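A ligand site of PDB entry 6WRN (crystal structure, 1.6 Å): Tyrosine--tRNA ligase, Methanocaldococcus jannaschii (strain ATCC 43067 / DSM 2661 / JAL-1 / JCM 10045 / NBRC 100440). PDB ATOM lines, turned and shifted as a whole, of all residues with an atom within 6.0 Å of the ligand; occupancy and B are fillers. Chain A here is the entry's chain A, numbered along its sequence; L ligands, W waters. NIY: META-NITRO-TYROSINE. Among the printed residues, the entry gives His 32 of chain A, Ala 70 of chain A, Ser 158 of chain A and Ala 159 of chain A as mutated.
OE1 of Gln 173 sits at hydrogen-bond distance from N of the ligand, 2.6 Å away.
The side-chain hydroxyl of Ser 158 is in hydrogen-bond range of an oxygen (OH) of the ligand (2.8 Å).
N of the ligand sits at hydrogen-bond distance from OE1 of Gln 155 (2.8 Å).
The side-chain hydroxyl (OH) of Tyr 151 sits at hydrogen-bond distance from a nitrogen (N) of the ligand (2.9 Å).
The side-chain amide nitrogen (NE2) of Gln 109 lies within hydrogen-bond range of an oxygen (O1) of the ligand, at 2.9 Å.
N of Glu 36 sits at hydrogen-bond distance from OXT of the ligand (3.0 Å).
OE1 of Gln 173 is in hydrogen-bond range of NE2 of Gln 155, 3.0 Å away.
OH of Tyr 114 is in hydrogen-bond range of N of Ser 158, 2.8 Å away.
The side-chain hydroxyl of Tyr 151 sits at hydrogen-bond distance from the side-chain carboxylate of Glu 36.
The side-chain sulfur of Met 154 lies close to the side-chain amide nitrogen of Gln 109, at 3.5 Å.
O of Leu 65 is in hydrogen-bond range of N of Phe 35 (3.0 Å).
O of Ile 33 lies within hydrogen-bond range of N of Leu 65 (2.9 Å).
The backbone NH of Ala 67 sits at hydrogen-bond distance from the backbone carbonyl oxygen of Phe 35.
The backbone carbonyl oxygen (O) of Met 154 sits at hydrogen-bond distance from the side-chain hydroxyl (OH) of Tyr 114 (2.7 Å).
Gly 34 touches the ligand (CA to CD2, 3.4 Å).
Phe 35 touches the ligand (CA to OXT, 3.7 Å).
CD2 of Leu 65 touches OH of the ligand, at 3.4 Å.
Ala 67 touches the ligand.
Ala 70 touches the ligand (CB to O2, 3.4 Å).
Met 154 touches the ligand (O to O1, 3.7 Å).
Hydrophobic or aromatic side chains that line the ligand: Leu 65, Ala 67, Ala 70 and Tyr 151.
Of the 22 residues printed, 12 come within 4 Å of the ligand.
The nearest printed residue that does not touch the ligand is His 32 (4.1 Å).
Water W3 lies within hydrogen-bond range of an oxygen (OH) of the ligand (2.7 Å), a ring nitrogen (NE2) of His 32 (3.1 Å) and the backbone carbonyl oxygen of Gln 155 (3.2 Å).
Water W6 lies within hydrogen-bond range of the side-chain amide oxygen of Gln 109, an oxygen (O2) of the ligand, the backbone NH of Ala 70 and the backbone NH of Leu 69.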
ATOM      1  N   HIS A  32     -25.840  11.782 -14.814  1.00  0.00           N
ATOM      2  CA  HIS A  32     -26.354  13.058 -15.350  1.00  0.00           C
ATOM      3  C   HIS A  32     -25.347  14.160 -15.346  1.00  0.00           C
ATOM      4  O   HIS A  32     -24.369  14.101 -14.695  1.00  0.00           O
ATOM      5  CB  HIS A  32     -27.684  13.521 -14.717  1.00  0.00           C
ATOM      6  CG  HIS A  32     -27.569  14.367 -13.484  1.00  0.00           C
ATOM      7  ND1 HIS A  32     -28.678  14.887 -12.871  1.00  0.00           N
ATOM      8  CD2 HIS A  32     -26.514  14.778 -12.744  1.00  0.00           C
ATOM      9  CE1 HIS A  32     -28.311  15.577 -11.805  1.00  0.00           C
ATOM     10  NE2 HIS A  32     -27.003  15.532 -11.718  1.00  0.00           N
ATOM     11  N   ILE A  33     -25.580  15.082 -16.240  1.00  0.00           N
ATOM     12  CA  ILE A  33     -24.824  16.325 -16.247  1.00  0.00           C
ATOM     13  C   ILE A  33     -25.851  17.411 -16.504  1.00  0.00           C
ATOM     14  O   ILE A  33     -26.816  17.226 -17.246  1.00  0.00           O
ATOM     15  CB  ILE A  33     -23.708  16.291 -17.324  1.00  0.00           C
ATOM     16  CG1 ILE A  33     -22.933  17.595 -17.367  1.00  0.00           C
ATOM     17  CG2 ILE A  33     -24.262  15.949 -18.697  1.00  0.00           C
ATOM     18  CD1 ILE A  33     -21.611  17.469 -18.036  1.00  0.00           C
ATOM     19  N   GLY A  34     -25.633  18.567 -15.913  1.00  0.00           N
ATOM     20  CA  GLY A  34     -26.486  19.719 -16.143  1.00  0.00           C
ATOM     21  C   GLY A  34     -25.692  20.807 -16.845  1.00  0.00           C
ATOM     22  O   GLY A  34     -24.499  20.994 -16.575  1.00  0.00           O
ATOM     23  N   PHE A  35     -26.375  21.527 -17.755  1.00  0.00           N
ATOM     24  CA  PHE A  35     -25.801  22.672 -18.437  1.00  0.00           C
ATOM     25  C   PHE A  35     -26.759  23.855 -18.364  1.00  0.00           C
ATOM     26  O   PHE A  35     -27.912  23.709 -18.748  1.00  0.00           O
ATOM     27  CB  PHE A  35     -25.554  22.418 -19.927  1.00  0.00           C
ATOM     28  CG  PHE A  35     -24.606  21.300 -20.236  1.00  0.00           C
ATOM     29  CD1 PHE A  35     -23.237  21.499 -20.149  1.00  0.00           C
ATOM     30  CD2 PHE A  35     -25.073  20.053 -20.690  1.00  0.00           C
ATOM     31  CE1 PHE A  35     -22.344  20.504 -20.509  1.00  0.00           C
ATOM     32  CE2 PHE A  35     -24.175  19.055 -21.038  1.00  0.00           C
ATOM     33  CZ  PHE A  35     -22.814  19.286 -20.932  1.00  0.00           C
ATOM     34  N   GLU A  36     -26.282  25.003 -17.864  1.00  0.00           N
ATOM     35  CA  GLU A  36     -26.990  26.245 -18.150  1.00  0.00           C
ATOM     36  C   GLU A  36     -27.070  26.382 -19.657  1.00  0.00           C
ATOM     37  O   GLU A  36     -26.051  26.262 -20.302  1.00  0.00           O
ATOM     38  CB  GLU A  36     -26.234  27.428 -17.597  1.00  0.00           C
ATOM     39  CG  GLU A  36     -26.172  27.406 -16.033  1.00  0.00           C
ATOM     40  CD  GLU A  36     -25.630  28.686 -15.479  1.00  0.00           C
ATOM     41  OE1 GLU A  36     -25.938  29.726 -16.082  1.00  0.00           O
ATOM     42  OE2 GLU A  36     -24.914  28.682 -14.431  1.00  0.00           O
ATOM     43  N   LEU A  65     -29.565  17.336 -18.069  1.00  0.00           N
ATOM     44  CA  LEU A  65     -30.387  18.370 -17.432  1.00  0.00           C
ATOM     45  C   LEU A  65     -30.123  19.694 -18.146  1.00  0.00           C
ATOM     46  O   LEU A  65     -29.005  20.206 -18.145  1.00  0.00           O
ATOM     47  CB  LEU A  65     -30.066  18.463 -15.948  1.00  0.00           C
ATOM     48  CG  LEU A  65     -30.700  19.622 -15.173  1.00  0.00           C
ATOM     49  CD1 LEU A  65     -32.208  19.502 -15.265  1.00  0.00           C
ATOM     50  CD2 LEU A  65     -30.248  19.602 -13.750  1.00  0.00           C
ATOM     51  N   ALA A  67     -30.493  23.130 -17.610  1.00  0.00           N
ATOM     52  CA  ALA A  67     -30.621  23.698 -16.260  1.00  0.00           C
ATOM     53  C   ALA A  67     -31.176  25.121 -16.356  1.00  0.00           C
ATOM     54  O   ALA A  67     -30.484  26.131 -16.120  1.00  0.00           O
ATOM     55  CB  ALA A  67     -29.281  23.671 -15.548  1.00  0.00           C
ATOM     56  N   LEU A  69     -33.562  26.741 -14.711  1.00  0.00           N
ATOM     57  CA  LEU A  69     -33.815  27.519 -13.488  1.00  0.00           C
ATOM     58  C   LEU A  69     -32.515  27.958 -12.864  1.00  0.00           C
ATOM     59  O   LEU A  69     -32.408  29.092 -12.385  1.00  0.00           O
ATOM     60  CB  LEU A  69     -34.664  26.712 -12.509  1.00  0.00           C
ATOM     61  CG  LEU A  69     -35.144  27.499 -11.289  1.00  0.00           C
ATOM     62  CD1 LEU A  69     -36.071  28.620 -11.649  1.00  0.00           C
ATOM     63  CD2 LEU A  69     -35.813  26.483 -10.375  1.00  0.00           C
ATOM     64  N   ALA A  70     -31.479  27.117 -12.932  1.00  0.00           N
ATOM     65  CA  ALA A  70     -30.152  27.535 -12.500  1.00  0.00           C
ATOM     66  C   ALA A  70     -29.686  28.711 -13.325  1.00  0.00           C
ATOM     67  O   ALA A  70     -29.122  29.666 -12.795  1.00  0.00           O
ATOM     68  CB  ALA A  70     -29.154  26.394 -12.591  1.00  0.00           C
ATOM     69  N   GLY A 105     -34.752  21.656 -15.746  1.00  0.00           N
ATOM     70  CA  GLY A 105     -34.775  21.771 -14.295  1.00  0.00           C
ATOM     71  C   GLY A 105     -36.139  22.171 -13.779  1.00  0.00           C
ATOM     72  O   GLY A 105     -36.642  21.594 -12.809  1.00  0.00           O
ATOM     73  N   GLN A 109     -37.946  21.291 -10.190  1.00  0.00           N
ATOM     74  CA  GLN A 109     -37.195  22.057  -9.152  1.00  0.00           C
ATOM     75  C   GLN A 109     -38.097  23.085  -8.447  1.00  0.00           C
ATOM     76  O   GLN A 109     -37.674  23.765  -7.553  1.00  0.00           O
ATOM     77  CB  GLN A 109     -35.912  22.732  -9.718  1.00  0.00           C
ATOM     78  CG  GLN A 109     -34.897  21.733 -10.279  1.00  0.00           C
ATOM     79  CD  GLN A 109     -33.674  22.430 -10.908  1.00  0.00           C
ATOM     80  OE1 GLN A 109     -33.831  23.338 -11.650  1.00  0.00           O
ATOM     81  NE2 GLN A 109     -32.489  21.972 -10.598  1.00  0.00           N
ATOM     82  N   TYR A 114     -39.427  19.501  -3.465  1.00  0.00           N
ATOM     83  CA  TYR A 114     -38.091  19.919  -3.865  1.00  0.00           C
ATOM     84  C   TYR A 114     -37.700  21.190  -3.099  1.00  0.00           C
ATOM     85  O   TYR A 114     -36.616  21.261  -2.486  1.00  0.00           O
ATOM     86  CB  TYR A 114     -38.035  20.175  -5.379  1.00  0.00           C
ATOM     87  CG  TYR A 114     -36.635  20.267  -5.926  1.00  0.00           C
ATOM     88  CD1 TYR A 114     -35.853  21.406  -5.776  1.00  0.00           C
ATOM     89  CD2 TYR A 114     -36.078  19.195  -6.622  1.00  0.00           C
ATOM     90  CE1 TYR A 114     -34.528  21.464  -6.296  1.00  0.00           C
ATOM     91  CE2 TYR A 114     -34.786  19.250  -7.142  1.00  0.00           C
ATOM     92  CZ  TYR A 114     -34.020  20.383  -6.987  1.00  0.00           C
ATOM     93  OH  TYR A 114     -32.721  20.388  -7.537  1.00  0.00           O
ATOM     94  N   ILE A 137     -18.392  29.843 -11.306  1.00  0.00           N
ATOM     95  CA  ILE A 137     -19.657  29.660 -12.002  1.00  0.00           C
ATOM     96  C   ILE A 137     -20.465  30.940 -12.058  1.00  0.00           C
ATOM     97  O   ILE A 137     -21.138  31.220 -13.060  1.00  0.00           O
ATOM     98  CB  ILE A 137     -20.481  28.559 -11.289  1.00  0.00           C
ATOM     99  CG1 ILE A 137     -19.794  27.204 -11.423  1.00  0.00           C
ATOM    100  CG2 ILE A 137     -21.913  28.521 -11.821  1.00  0.00           C
ATOM    101  CD1 ILE A 137     -20.301  26.159 -10.433  1.00  0.00           C
ATOM    102  N   TYR A 151     -28.424  29.016  -5.898  1.00  0.00           N
ATOM    103  CA  TYR A 151     -27.968  28.151  -6.989  1.00  0.00           C
ATOM    104  C   TYR A 151     -27.246  26.909  -6.519  1.00  0.00           C
ATOM    105  O   TYR A 151     -27.625  25.812  -6.943  1.00  0.00           O
ATOM    106  CB  TYR A 151     -27.090  29.027  -7.894  1.00  0.00           C
ATOM    107  CG  TYR A 151     -26.559  28.397  -9.160  1.00  0.00           C
ATOM    108  CD1 TYR A 151     -25.666  27.326  -9.139  1.00  0.00           C
ATOM    109  CD2 TYR A 151     -26.885  28.926 -10.381  1.00  0.00           C
ATOM    110  CE1 TYR A 151     -25.133  26.802 -10.319  1.00  0.00           C
ATOM    111  CE2 TYR A 151     -26.361  28.426 -11.576  1.00  0.00           C
ATOM    112  CZ  TYR A 151     -25.489  27.349 -11.530  1.00  0.00           C
ATOM    113  OH  TYR A 151     -24.953  26.834 -12.710  1.00  0.00           O
ATOM    114  N   MET A 154     -29.732  24.457  -5.040  1.00  0.00           N
ATOM    115  CA  MET A 154     -30.511  23.879  -6.120  1.00  0.00           C
ATOM    116  C   MET A 154     -29.780  22.711  -6.735  1.00  0.00           C
ATOM    117  O   MET A 154     -30.361  21.637  -6.933  1.00  0.00           O
ATOM    118  CB  MET A 154     -30.810  24.985  -7.143  1.00  0.00           C
ATOM    119  CG  MET A 154     -31.575  24.560  -8.355  1.00  0.00           C
ATOM    120  SD  MET A 154     -33.238  24.062  -7.939  1.00  0.00           S
ATOM    121  CE  MET A 154     -33.940  25.546  -7.230  1.00  0.00           C
ATOM    122  N   GLN A 155     -28.495  22.872  -7.015  1.00  0.00           N
ATOM    123  CA  GLN A 155     -27.750  21.821  -7.700  1.00  0.00           C
ATOM    124  C   GLN A 155     -27.436  20.627  -6.799  1.00  0.00           C
ATOM    125  O   GLN A 155     -27.448  19.479  -7.277  1.00  0.00           O
ATOM    126  CB  GLN A 155     -26.459  22.404  -8.305  1.00  0.00           C
ATOM    127  CG  GLN A 155     -25.611  21.394  -9.061  1.00  0.00           C
ATOM    128  CD  GLN A 155     -24.563  22.124  -9.887  1.00  0.00           C
ATOM    129  OE1 GLN A 155     -24.739  23.298 -10.181  1.00  0.00           O
ATOM    130  NE2 GLN A 155     -23.438  21.447 -10.200  1.00  0.00           N
ATOM    131  N   VAL A 156     -27.188  20.850  -5.499  1.00  0.00           N
ATOM    132  CA  VAL A 156     -27.024  19.745  -4.565  1.00  0.00           C
ATOM    133  C   VAL A 156     -28.274  18.882  -4.547  1.00  0.00           C
ATOM    134  O   VAL A 156     -28.210  17.658  -4.640  1.00  0.00           O
ATOM    135  CB  VAL A 156     -26.684  20.277  -3.170  1.00  0.00           C
ATOM    136  CG1 VAL A 156     -26.765  19.133  -2.098  1.00  0.00           C
ATOM    137  CG2 VAL A 156     -25.280  20.879  -3.156  1.00  0.00           C
ATOM    138  N   SER A 158     -30.639  18.622  -6.781  1.00  0.00           N
ATOM    139  CA  SER A 158     -30.844  18.006  -8.098  1.00  0.00           C
ATOM    140  C   SER A 158     -30.374  16.516  -8.168  1.00  0.00           C
ATOM    141  O   SER A 158     -31.048  15.636  -8.630  1.00  0.00           O
ATOM    142  CB  SER A 158     -30.146  18.778  -9.276  1.00  0.00           C
ATOM    143  OG  SER A 158     -30.342  18.230 -10.463  1.00  0.00           O
ATOM    144  N   ALA A 159     -29.150  16.301  -7.792  1.00  0.00           N
ATOM    145  CA  ALA A 159     -28.576  14.966  -7.806  1.00  0.00           C
ATOM    146  C   ALA A 159     -29.331  14.032  -6.858  1.00  0.00           C
ATOM    147  O   ALA A 159     -29.597  12.878  -7.212  1.00  0.00           O
ATOM    148  CB  ALA A 159     -27.103  15.057  -7.408  1.00  0.00           C
ATOM    149  N   GLN A 173     -17.278  22.699 -11.171  1.00  0.00           N
ATOM    150  CA  GLN A 173     -18.385  22.216 -10.376  1.00  0.00           C
ATOM    151  C   GLN A 173     -17.942  21.525  -9.093  1.00  0.00           C
ATOM    152  O   GLN A 173     -18.800  21.091  -8.308  1.00  0.00           O
ATOM    153  CB  GLN A 173     -19.222  21.234 -11.189  1.00  0.00           C
ATOM    154  CG  GLN A 173     -19.625  21.706 -12.585  1.00  0.00           C
ATOM    155  CD  GLN A 173     -20.527  22.903 -12.599  1.00  0.00           C
ATOM    156  OE1 GLN A 173     -21.499  22.980 -11.843  1.00  0.00           O
ATOM    157  NE2 GLN A 173     -20.236  23.851 -13.494  1.00  0.00           N
ATOM    158  N   ILE A 176     -19.287  22.556  -5.485  1.00  0.00           N
ATOM    159  CA  ILE A 176     -20.697  22.198  -5.301  1.00  0.00           C
ATOM    160  C   ILE A 176     -20.833  20.699  -5.082  1.00  0.00           C
ATOM    161  O   ILE A 176     -21.628  20.233  -4.254  1.00  0.00           O
ATOM    162  CB  ILE A 176     -21.565  22.640  -6.486  1.00  0.00           C
ATOM    163  CG1 ILE A 176     -21.702  24.159  -6.566  1.00  0.00           C
ATOM    164  CG2 ILE A 176     -22.938  21.982  -6.415  1.00  0.00           C
ATOM    165  CD1 ILE A 176     -22.362  24.685  -7.806  1.00  0.00           C
ATOM    166  N   HIS A 177     -20.076  19.890  -5.847  1.00  0.00           N
ATOM    167  CA  HIS A 177     -20.200  18.437  -5.719  1.00  0.00           C
ATOM    168  C   HIS A 177     -19.677  17.948  -4.367  1.00  0.00           C
ATOM    169  O   HIS A 177     -20.253  17.029  -3.770  1.00  0.00           O
ATOM    170  CB  HIS A 177     -19.473  17.754  -6.865  1.00  0.00           C
ATOM    171  CG  HIS A 177     -20.235  17.813  -8.150  1.00  0.00           C
ATOM    172  ND1 HIS A 177     -19.671  17.502  -9.363  1.00  0.00           N
ATOM    173  CD2 HIS A 177     -21.524  18.137  -8.401  1.00  0.00           C
ATOM    174  CE1 HIS A 177     -20.582  17.623 -10.319  1.00  0.00           C
ATOM    175  NE2 HIS A 177     -21.714  18.030  -9.766  1.00  0.00           N
HETATM  176  N   NIY L   1     -23.678  24.233 -12.631  1.00  0.00           N
HETATM  177  CA  NIY L   1     -23.950  23.799 -14.044  1.00  0.00           C
HETATM  178  C   NIY L   1     -23.344  24.785 -15.022  1.00  0.00           C
HETATM  179  O   NIY L   1     -22.418  25.530 -14.611  1.00  0.00           O
HETATM  180  CB  NIY L   1     -25.455  23.678 -14.241  1.00  0.00           C
HETATM  181  CG  NIY L   1     -26.149  22.584 -13.420  1.00  0.00           C
HETATM  182  CD1 NIY L   1     -27.350  22.857 -12.785  1.00  0.00           C
HETATM  183  CD2 NIY L   1     -25.566  21.317 -13.304  1.00  0.00           C
HETATM  184  CE1 NIY L   1     -27.976  21.856 -12.047  1.00  0.00           C
HETATM  185  CE2 NIY L   1     -26.174  20.323 -12.581  1.00  0.00           C
HETATM  186  CZ  NIY L   1     -27.385  20.609 -11.938  1.00  0.00           C
HETATM  187  OH  NIY L   1     -28.027  19.635 -11.227  1.00  0.00           O
HETATM  188  NN  NIY L   1     -29.182  22.161 -11.402  1.00  0.00           N
HETATM  189  O1  NIY L   1     -29.601  21.435 -10.519  1.00  0.00           O
HETATM  190  O2  NIY L   1     -29.823  23.152 -11.749  1.00  0.00           O
HETATM  191  OXT NIY L   1     -23.750  24.792 -16.206  1.00  0.00           O
HETATM  192  O   HOH W   1     -24.067  18.124 -11.119  1.00  0.00           O
HETATM  193  O   HOH W   2     -22.114  25.056 -18.321  1.00  0.00           O
HETATM  194  O   HOH W   3     -26.441  17.927  -9.869  1.00  0.00           O
HETATM  195  O   HOH W   4     -22.361  20.829 -14.946  1.00  0.00           O
HETATM  196  O   HOH W   5     -20.954  27.481 -15.688  1.00  0.00           O
HETATM  197  O   HOH W   6     -31.943  24.246 -13.362  1.00  0.00           O
